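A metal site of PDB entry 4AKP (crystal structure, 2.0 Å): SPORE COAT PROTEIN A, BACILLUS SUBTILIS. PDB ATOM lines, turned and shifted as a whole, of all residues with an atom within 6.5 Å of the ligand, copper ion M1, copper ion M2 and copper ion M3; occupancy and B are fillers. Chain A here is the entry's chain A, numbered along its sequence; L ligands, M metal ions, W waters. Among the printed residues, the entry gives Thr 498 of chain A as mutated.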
ATOM      1  N   HIS A 105       1.203  -7.403  20.811  1.00  0.00           N
ATOM      2  CA  HIS A 105       2.142  -6.921  19.825  1.00  0.00           C
ATOM      3  C   HIS A 105       1.472  -6.885  18.447  1.00  0.00           C
ATOM      4  O   HIS A 105       0.952  -7.908  17.989  1.00  0.00           O
ATOM      5  CB  HIS A 105       3.373  -7.834  19.768  1.00  0.00           C
ATOM      6  CG  HIS A 105       4.299  -7.554  18.618  1.00  0.00           C
ATOM      7  ND1 HIS A 105       4.885  -6.315  18.416  1.00  0.00           N
ATOM      8  CD2 HIS A 105       4.746  -8.349  17.622  1.00  0.00           C
ATOM      9  CE1 HIS A 105       5.647  -6.368  17.345  1.00  0.00           C
ATOM     10  NE2 HIS A 105       5.588  -7.581  16.842  1.00  0.00           N
ATOM     11  N   LEU A 106       1.492  -5.715  17.816  1.00  0.00           N
ATOM     12  CA  LEU A 106       1.116  -5.599  16.404  1.00  0.00           C
ATOM     13  C   LEU A 106       2.312  -5.944  15.517  1.00  0.00           C
ATOM     14  O   LEU A 106       3.205  -5.108  15.310  1.00  0.00           O
ATOM     15  CB  LEU A 106       0.579  -4.208  16.076  1.00  0.00           C
ATOM     16  CG  LEU A 106       0.161  -3.990  14.610  1.00  0.00           C
ATOM     17  CD1 LEU A 106      -0.965  -4.937  14.202  1.00  0.00           C
ATOM     18  CD2 LEU A 106      -0.261  -2.555  14.369  1.00  0.00           C
ATOM     19  N   HIS A 107       2.318  -7.179  15.013  1.00  0.00           N
ATOM     20  CA  HIS A 107       3.426  -7.723  14.245  1.00  0.00           C
ATOM     21  C   HIS A 107       3.516  -7.054  12.879  1.00  0.00           C
ATOM     22  O   HIS A 107       2.569  -7.110  12.088  1.00  0.00           O
ATOM     23  CB  HIS A 107       3.256  -9.230  14.097  1.00  0.00           C
ATOM     24  CG  HIS A 107       4.422  -9.930  13.481  1.00  0.00           C
ATOM     25  ND1 HIS A 107       5.176 -10.871  14.147  1.00  0.00           N
ATOM     26  CD2 HIS A 107       4.967  -9.813  12.242  1.00  0.00           C
ATOM     27  CE1 HIS A 107       6.117 -11.322  13.335  1.00  0.00           C
ATOM     28  NE2 HIS A 107       6.025 -10.692  12.185  1.00  0.00           N
ATOM     29  N   GLY A 108       4.661  -6.412  12.618  1.00  0.00           N
ATOM     30  CA  GLY A 108       4.851  -5.607  11.397  1.00  0.00           C
ATOM     31  C   GLY A 108       4.548  -4.136  11.616  1.00  0.00           C
ATOM     32  O   GLY A 108       4.744  -3.300  10.712  1.00  0.00           O
ATOM     33  N   GLY A 109       4.043  -3.800  12.799  1.00  0.00           N
ATOM     34  CA  GLY A 109       3.658  -2.411  13.088  1.00  0.00           C
ATOM     35  C   GLY A 109       4.872  -1.504  13.169  1.00  0.00           C
ATOM     36  O   GLY A 109       5.846  -1.809  13.854  1.00  0.00           O
ATOM     37  N   ASP A 116       4.563  -1.039  21.232  1.00  0.00           N
ATOM     38  CA  ASP A 116       4.982  -2.207  20.439  1.00  0.00           C
ATOM     39  C   ASP A 116       4.667  -3.559  21.113  1.00  0.00           C
ATOM     40  O   ASP A 116       4.715  -4.614  20.459  1.00  0.00           O
ATOM     41  CB  ASP A 116       6.485  -2.106  20.103  1.00  0.00           C
ATOM     42  CG  ASP A 116       6.917  -3.094  19.016  1.00  0.00           C
ATOM     43  OD1 ASP A 116       6.218  -3.202  17.993  1.00  0.00           O
ATOM     44  OD2 ASP A 116       7.967  -3.753  19.200  1.00  0.00           O
ATOM     45  N   TRP A 151      -0.504  -8.593  11.704  1.00  0.00           N
ATOM     46  CA  TRP A 151      -1.309  -9.426  12.580  1.00  0.00           C
ATOM     47  C   TRP A 151      -0.920  -9.112  14.004  1.00  0.00           C
ATOM     48  O   TRP A 151       0.180  -8.621  14.267  1.00  0.00           O
ATOM     49  CB  TRP A 151      -1.191 -10.918  12.237  1.00  0.00           C
ATOM     50  CG  TRP A 151       0.150 -11.588  12.493  1.00  0.00           C
ATOM     51  CD1 TRP A 151       1.368 -11.276  11.924  1.00  0.00           C
ATOM     52  CD2 TRP A 151       0.395 -12.707  13.361  1.00  0.00           C
ATOM     53  NE1 TRP A 151       2.334 -12.127  12.389  1.00  0.00           N
ATOM     54  CE2 TRP A 151       1.769 -13.010  13.271  1.00  0.00           C
ATOM     55  CE3 TRP A 151      -0.422 -13.481  14.201  1.00  0.00           C
ATOM     56  CZ2 TRP A 151       2.356 -14.046  14.016  1.00  0.00           C
ATOM     57  CZ3 TRP A 151       0.160 -14.515  14.933  1.00  0.00           C
ATOM     58  CH2 TRP A 151       1.540 -14.787  14.831  1.00  0.00           C
ATOM     59  N   HIS A 153      -0.845 -10.339  18.171  1.00  0.00           N
ATOM     60  CA  HIS A 153      -0.783 -11.524  18.999  1.00  0.00           C
ATOM     61  C   HIS A 153      -0.198 -11.188  20.370  1.00  0.00           C
ATOM     62  O   HIS A 153       0.421 -10.127  20.545  1.00  0.00           O
ATOM     63  CB  HIS A 153      -0.006 -12.670  18.304  1.00  0.00           C
ATOM     64  CG  HIS A 153       1.445 -12.367  18.004  1.00  0.00           C
ATOM     65  ND1 HIS A 153       2.451 -12.538  18.932  1.00  0.00           N
ATOM     66  CD2 HIS A 153       2.061 -11.986  16.856  1.00  0.00           C
ATOM     67  CE1 HIS A 153       3.612 -12.237  18.384  1.00  0.00           C
ATOM     68  NE2 HIS A 153       3.414 -11.907  17.117  1.00  0.00           N
ATOM     69  N   ASP A 154      -0.415 -12.067  21.328  1.00  0.00           N
ATOM     70  CA  ASP A 154       0.154 -11.872  22.651  1.00  0.00           C
ATOM     71  C   ASP A 154       1.682 -11.997  22.599  1.00  0.00           C
ATOM     72  O   ASP A 154       2.199 -12.815  21.851  1.00  0.00           O
ATOM     73  CB  ASP A 154      -0.408 -12.871  23.655  1.00  0.00           C
ATOM     74  CG  ASP A 154       0.000 -12.536  25.069  1.00  0.00           C
ATOM     75  OD1 ASP A 154      -0.570 -11.571  25.629  1.00  0.00           O
ATOM     76  OD2 ASP A 154       0.931 -13.182  25.586  1.00  0.00           O
ATOM     77  N   HIS A 155       2.383 -11.208  23.406  1.00  0.00           N
ATOM     78  CA  HIS A 155       3.842 -11.205  23.411  1.00  0.00           C
ATOM     79  C   HIS A 155       4.428 -11.248  24.846  1.00  0.00           C
ATOM     80  O   HIS A 155       5.566 -10.831  25.053  1.00  0.00           O
ATOM     81  CB  HIS A 155       4.388  -9.973  22.654  1.00  0.00           C
ATOM     82  CG  HIS A 155       5.630 -10.250  21.842  1.00  0.00           C
ATOM     83  ND1 HIS A 155       6.796 -10.733  22.384  1.00  0.00           N
ATOM     84  CD2 HIS A 155       5.879 -10.084  20.517  1.00  0.00           C
ATOM     85  CE1 HIS A 155       7.706 -10.854  21.440  1.00  0.00           C
ATOM     86  NE2 HIS A 155       7.177 -10.468  20.284  1.00  0.00           N
ATOM     87  N   THR A 160       4.384 -16.492  25.698  1.00  0.00           N
ATOM     88  CA  THR A 160       3.930 -16.273  24.326  1.00  0.00           C
ATOM     89  C   THR A 160       3.421 -17.565  23.663  1.00  0.00           C
ATOM     90  O   THR A 160       2.387 -17.552  22.993  1.00  0.00           O
ATOM     91  CB  THR A 160       5.038 -15.568  23.484  1.00  0.00           C
ATOM     92  OG1 THR A 160       5.373 -14.320  24.099  1.00  0.00           O
ATOM     93  CG2 THR A 160       4.597 -15.305  22.060  1.00  0.00           C
ATOM     94  N   ALA A 297       4.705 -16.745  11.441  1.00  0.00           N
ATOM     95  CA  ALA A 297       4.701 -15.272  11.363  1.00  0.00           C
ATOM     96  C   ALA A 297       4.921 -14.672   9.976  1.00  0.00           C
ATOM     97  O   ALA A 297       4.745 -13.466   9.801  1.00  0.00           O
ATOM     98  CB  ALA A 297       5.672 -14.660  12.386  1.00  0.00           C
ATOM     99  N   HIS A 422      12.805 -12.759  13.226  1.00  0.00           N
ATOM    100  CA  HIS A 422      11.955 -11.603  13.133  1.00  0.00           C
ATOM    101  C   HIS A 422      12.565 -10.415  13.863  1.00  0.00           C
ATOM    102  O   HIS A 422      13.049 -10.552  14.992  1.00  0.00           O
ATOM    103  CB  HIS A 422      10.581 -11.951  13.719  1.00  0.00           C
ATOM    104  CG  HIS A 422       9.643 -10.785  13.829  1.00  0.00           C
ATOM    105  ND1 HIS A 422       9.356  -9.966  12.762  1.00  0.00           N
ATOM    106  CD2 HIS A 422       8.944 -10.301  14.875  1.00  0.00           C
ATOM    107  CE1 HIS A 422       8.514  -9.017  13.143  1.00  0.00           C
ATOM    108  NE2 HIS A 422       8.254  -9.202  14.421  1.00  0.00           N
ATOM    109  N   LEU A 423      12.528  -9.254  13.199  1.00  0.00           N
ATOM    110  CA  LEU A 423      12.914  -7.969  13.778  1.00  0.00           C
ATOM    111  C   LEU A 423      11.673  -7.110  13.945  1.00  0.00           C
ATOM    112  O   LEU A 423      10.917  -6.914  12.989  1.00  0.00           O
ATOM    113  CB  LEU A 423      13.922  -7.250  12.879  1.00  0.00           C
ATOM    114  CG  LEU A 423      15.413  -7.603  12.995  1.00  0.00           C
ATOM    115  CD1 LEU A 423      15.709  -9.071  12.685  1.00  0.00           C
ATOM    116  CD2 LEU A 423      16.241  -6.688  12.089  1.00  0.00           C
ATOM    117  N   HIS A 424      11.465  -6.580  15.142  1.00  0.00           N
ATOM    118  CA  HIS A 424      10.386  -5.621  15.373  1.00  0.00           C
ATOM    119  C   HIS A 424      10.700  -4.310  14.652  1.00  0.00           C
ATOM    120  O   HIS A 424      11.834  -4.097  14.205  1.00  0.00           O
ATOM    121  CB  HIS A 424      10.163  -5.395  16.876  1.00  0.00           C
ATOM    122  CG  HIS A 424       9.471  -6.524  17.560  1.00  0.00           C
ATOM    123  ND1 HIS A 424       8.588  -6.331  18.611  1.00  0.00           N
ATOM    124  CD2 HIS A 424       9.526  -7.869  17.363  1.00  0.00           C
ATOM    125  CE1 HIS A 424       8.136  -7.506  19.021  1.00  0.00           C
ATOM    126  NE2 HIS A 424       8.683  -8.458  18.278  1.00  0.00           N
ATOM    127  N   LEU A 425       9.666  -3.473  14.516  1.00  0.00           N
ATOM    128  CA  LEU A 425       9.710  -2.132  13.922  1.00  0.00           C
ATOM    129  C   LEU A 425       9.910  -2.066  12.415  1.00  0.00           C
ATOM    130  O   LEU A 425       9.148  -1.406  11.706  1.00  0.00           O
ATOM    131  CB  LEU A 425      10.712  -1.194  14.629  1.00  0.00           C
ATOM    132  CG  LEU A 425      10.736   0.263  14.130  1.00  0.00           C
ATOM    133  CD1 LEU A 425       9.401   0.968  14.372  1.00  0.00           C
ATOM    134  CD2 LEU A 425      11.890   1.066  14.721  1.00  0.00           C
ATOM    135  N   ASP A 465       9.815  -9.090   7.147  1.00  0.00           N
ATOM    136  CA  ASP A 465      10.115  -8.832   8.573  1.00  0.00           C
ATOM    137  C   ASP A 465      10.364 -10.121   9.339  1.00  0.00           C
ATOM    138  O   ASP A 465      10.817 -10.091  10.479  1.00  0.00           O
ATOM    139  CB  ASP A 465       9.079  -7.903   9.241  1.00  0.00           C
ATOM    140  CG  ASP A 465       7.684  -8.538   9.374  1.00  0.00           C
ATOM    141  OD1 ASP A 465       7.570  -9.729   9.734  1.00  0.00           O
ATOM    142  OD2 ASP A 465       6.705  -7.806   9.146  1.00  0.00           O
ATOM    143  N   THR A 466      10.072 -11.249   8.710  1.00  0.00           N
ATOM    144  CA  THR A 466      10.287 -12.561   9.297  1.00  0.00           C
ATOM    145  C   THR A 466      10.893 -13.423   8.197  1.00  0.00           C
ATOM    146  O   THR A 466      10.304 -13.558   7.130  1.00  0.00           O
ATOM    147  CB  THR A 466       8.976 -13.206   9.807  1.00  0.00           C
ATOM    148  OG1 THR A 466       8.316 -12.314  10.725  1.00  0.00           O
ATOM    149  CG2 THR A 466       9.263 -14.526  10.512  1.00  0.00           C
ATOM    150  N   VAL A 489      12.676  -5.477  20.067  1.00  0.00           N
ATOM    151  CA  VAL A 489      13.216  -6.823  20.215  1.00  0.00           C
ATOM    152  C   VAL A 489      13.452  -7.467  18.864  1.00  0.00           C
ATOM    153  O   VAL A 489      12.920  -7.018  17.848  1.00  0.00           O
ATOM    154  CB  VAL A 489      12.341  -7.774  21.117  1.00  0.00           C
ATOM    155  CG1 VAL A 489      12.017  -7.149  22.469  1.00  0.00           C
ATOM    156  CG2 VAL A 489      11.057  -8.196  20.415  1.00  0.00           C
ATOM    157  N   HIS A 491      13.916 -11.745  17.485  1.00  0.00           N
ATOM    158  CA  HIS A 491      13.799 -13.112  17.987  1.00  0.00           C
ATOM    159  C   HIS A 491      13.492 -14.130  16.903  1.00  0.00           C
ATOM    160  O   HIS A 491      13.100 -13.782  15.791  1.00  0.00           O
ATOM    161  CB  HIS A 491      12.729 -13.216  19.088  1.00  0.00           C
ATOM    162  CG  HIS A 491      11.363 -12.735  18.691  1.00  0.00           C
ATOM    163  ND1 HIS A 491      10.363 -13.585  18.261  1.00  0.00           N
ATOM    164  CD2 HIS A 491      10.829 -11.488  18.690  1.00  0.00           C
ATOM    165  CE1 HIS A 491       9.271 -12.885  18.002  1.00  0.00           C
ATOM    166  NE2 HIS A 491       9.521 -11.615  18.259  1.00  0.00           N
ATOM    167  N   HIS A 493      10.785 -16.707  15.671  1.00  0.00           N
ATOM    168  CA  HIS A 493       9.325 -16.701  15.817  1.00  0.00           C
ATOM    169  C   HIS A 493       8.711 -18.111  15.945  1.00  0.00           C
ATOM    170  O   HIS A 493       7.503 -18.286  15.806  1.00  0.00           O
ATOM    171  CB  HIS A 493       8.631 -15.886  14.715  1.00  0.00           C
ATOM    172  CG  HIS A 493       7.458 -15.076  15.203  1.00  0.00           C
ATOM    173  ND1 HIS A 493       6.299 -15.661  15.679  1.00  0.00           N
ATOM    174  CD2 HIS A 493       7.264 -13.731  15.278  1.00  0.00           C
ATOM    175  CE1 HIS A 493       5.446 -14.706  16.034  1.00  0.00           C
ATOM    176  NE2 HIS A 493       6.004 -13.531  15.798  1.00  0.00           N
ATOM    177  N   LEU A 495       7.674 -20.118  18.696  1.00  0.00           N
ATOM    178  CA  LEU A 495       7.348 -19.590  20.027  1.00  0.00           C
ATOM    179  C   LEU A 495       7.949 -20.414  21.166  1.00  0.00           C
ATOM    180  O   LEU A 495       8.288 -19.864  22.218  1.00  0.00           O
ATOM    181  CB  LEU A 495       5.833 -19.412  20.180  1.00  0.00           C
ATOM    182  CG  LEU A 495       5.199 -18.491  19.132  1.00  0.00           C
ATOM    183  CD1 LEU A 495       3.726 -18.310  19.408  1.00  0.00           C
ATOM    184  CD2 LEU A 495       5.906 -17.128  19.048  1.00  0.00           C
ATOM    185  N   THR A 498      11.284 -18.866  21.213  1.00  0.00           N
ATOM    186  CA  THR A 498      11.152 -17.493  21.714  1.00  0.00           C
ATOM    187  C   THR A 498      11.173 -17.437  23.242  1.00  0.00           C
ATOM    188  O   THR A 498      11.855 -16.588  23.843  1.00  0.00           O
ATOM    189  CB  THR A 498       9.846 -16.827  21.208  1.00  0.00           C
ATOM    190  OG1 THR A 498       9.686 -17.077  19.804  1.00  0.00           O
ATOM    191  CG2 THR A 498       9.890 -15.328  21.445  1.00  0.00           C
ATOM    192  N   MET A 503      15.410 -14.774  22.178  1.00  0.00           N
ATOM    193  CA  MET A 503      14.902 -13.427  22.000  1.00  0.00           C
ATOM    194  C   MET A 503      15.848 -12.462  22.674  1.00  0.00           C
ATOM    195  O   MET A 503      16.309 -12.724  23.785  1.00  0.00           O
ATOM    196  CB  MET A 503      13.496 -13.310  22.595  1.00  0.00           C
ATOM    197  CG  MET A 503      12.877 -11.936  22.461  1.00  0.00           C
ATOM    198  SD  MET A 503      11.149 -11.857  22.993  1.00  0.00           S
ATOM    199  CE  MET A 503      11.309 -12.245  24.739  1.00  0.00           C
HETATM  200  O1  LIG L   1       6.631 -10.422  16.738  1.00  0.00           O
HETATM  201  O2  LIG L   1       6.491 -11.271  17.389  1.00  0.00           O
HETATM  202 CU    CU M   1       7.987 -10.334  18.438  1.00  0.00          CU
HETATM  203 CU    CU M   2       5.069 -11.737  15.953  1.00  0.00          CU
HETATM  204 CU    CU M   3       6.819  -8.625  15.669  1.00  0.00          CU
HETATM  205  O   HOH W   1       6.929  -5.900  14.018  1.00  0.00           O
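Copper ion M1 is bound by NE2 of His 491 (2.0 Å), NE2 of His 424 (2.0 Å), NE2 of His 155 (2.0 Å) and O2 of the ligand (2.1 Å). Copper ion M1 has four donor atoms within binding distance.
Within 4 Å of copper ion M2: His 105, His 107, His 153 and His 493. The nearest printed residue that does not touch copper ion M2 is Trp 151 (4.1 Å).
Four residues have an atom within 4 Å of copper ion M3: His 105, His 107, His 422 and His 424. Along chain A the residues within 4 Å of copper ion M3 span positions 105 to 424. The nearest printed residue that does not touch copper ion M3 is Gly 108 (4.3 Å).
Hydrophobic or aromatic side chains within 4 Å of the ligand: His 105, His 107, His 153, His 155, His 422, His 424, His 491 and His 493. The nearest printed residue that does not touch the ligand is Trp 151 (6.0 Å).
Copper ion M3 is bound by a ring nitrogen (NE2) of His 422, a ring nitrogen (NE2) of His 105 and an oxygen (O1) of the ligand. Copper ion M3 has three donor atoms within binding distance.
Five residues have an atom within 4 Å of copper ion M1: His 105, His 155, His 422, His 424 and His 491. The nearest printed residue that does not touch copper ion M1 is Val 489 (4.2 Å).
Copper ion M2 is bound by a ring nitrogen (ND1) of His 107 (2.0 Å), a ring nitrogen (NE2) of His 493 (2.0 Å), a ring nitrogen (NE2) of His 153 (2.0 Å) and an oxygen (O2) of the ligand (2.1 Å). Copper ion M2 has four donor atoms within binding distance.
The backbone NH (N) of His 424 sits at hydrogen-bond distance from the backbone carbonyl oxygen (O) of Val 489, 3.1 Å away. O of His 153 sits at hydrogen-bond distance from N of His 105 (2.8 Å). ND1 of His 422 sits at hydrogen-bond distance from O of Asp 465, 2.7 Å away. O of Asp 116 is in hydrogen-bond range of ND1 of His 105, 2.7 Å away. A ring nitrogen (NE2) of His 107 is in hydrogen-bond range of the side-chain hydroxyl (OG1) of Thr 466, at 3.2 Å. OG1 of Thr 466 sits at hydrogen-bond distance from ND1 of His 422, at 3.3 Å. The backbone NH (N) of His 107 is in hydrogen-bond range of the backbone carbonyl oxygen (O) of Trp 151. A ring nitrogen (ND1) of His 424 lies within hydrogen-bond range of the side-chain carboxylate of Asp 116 (2.7 Å).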
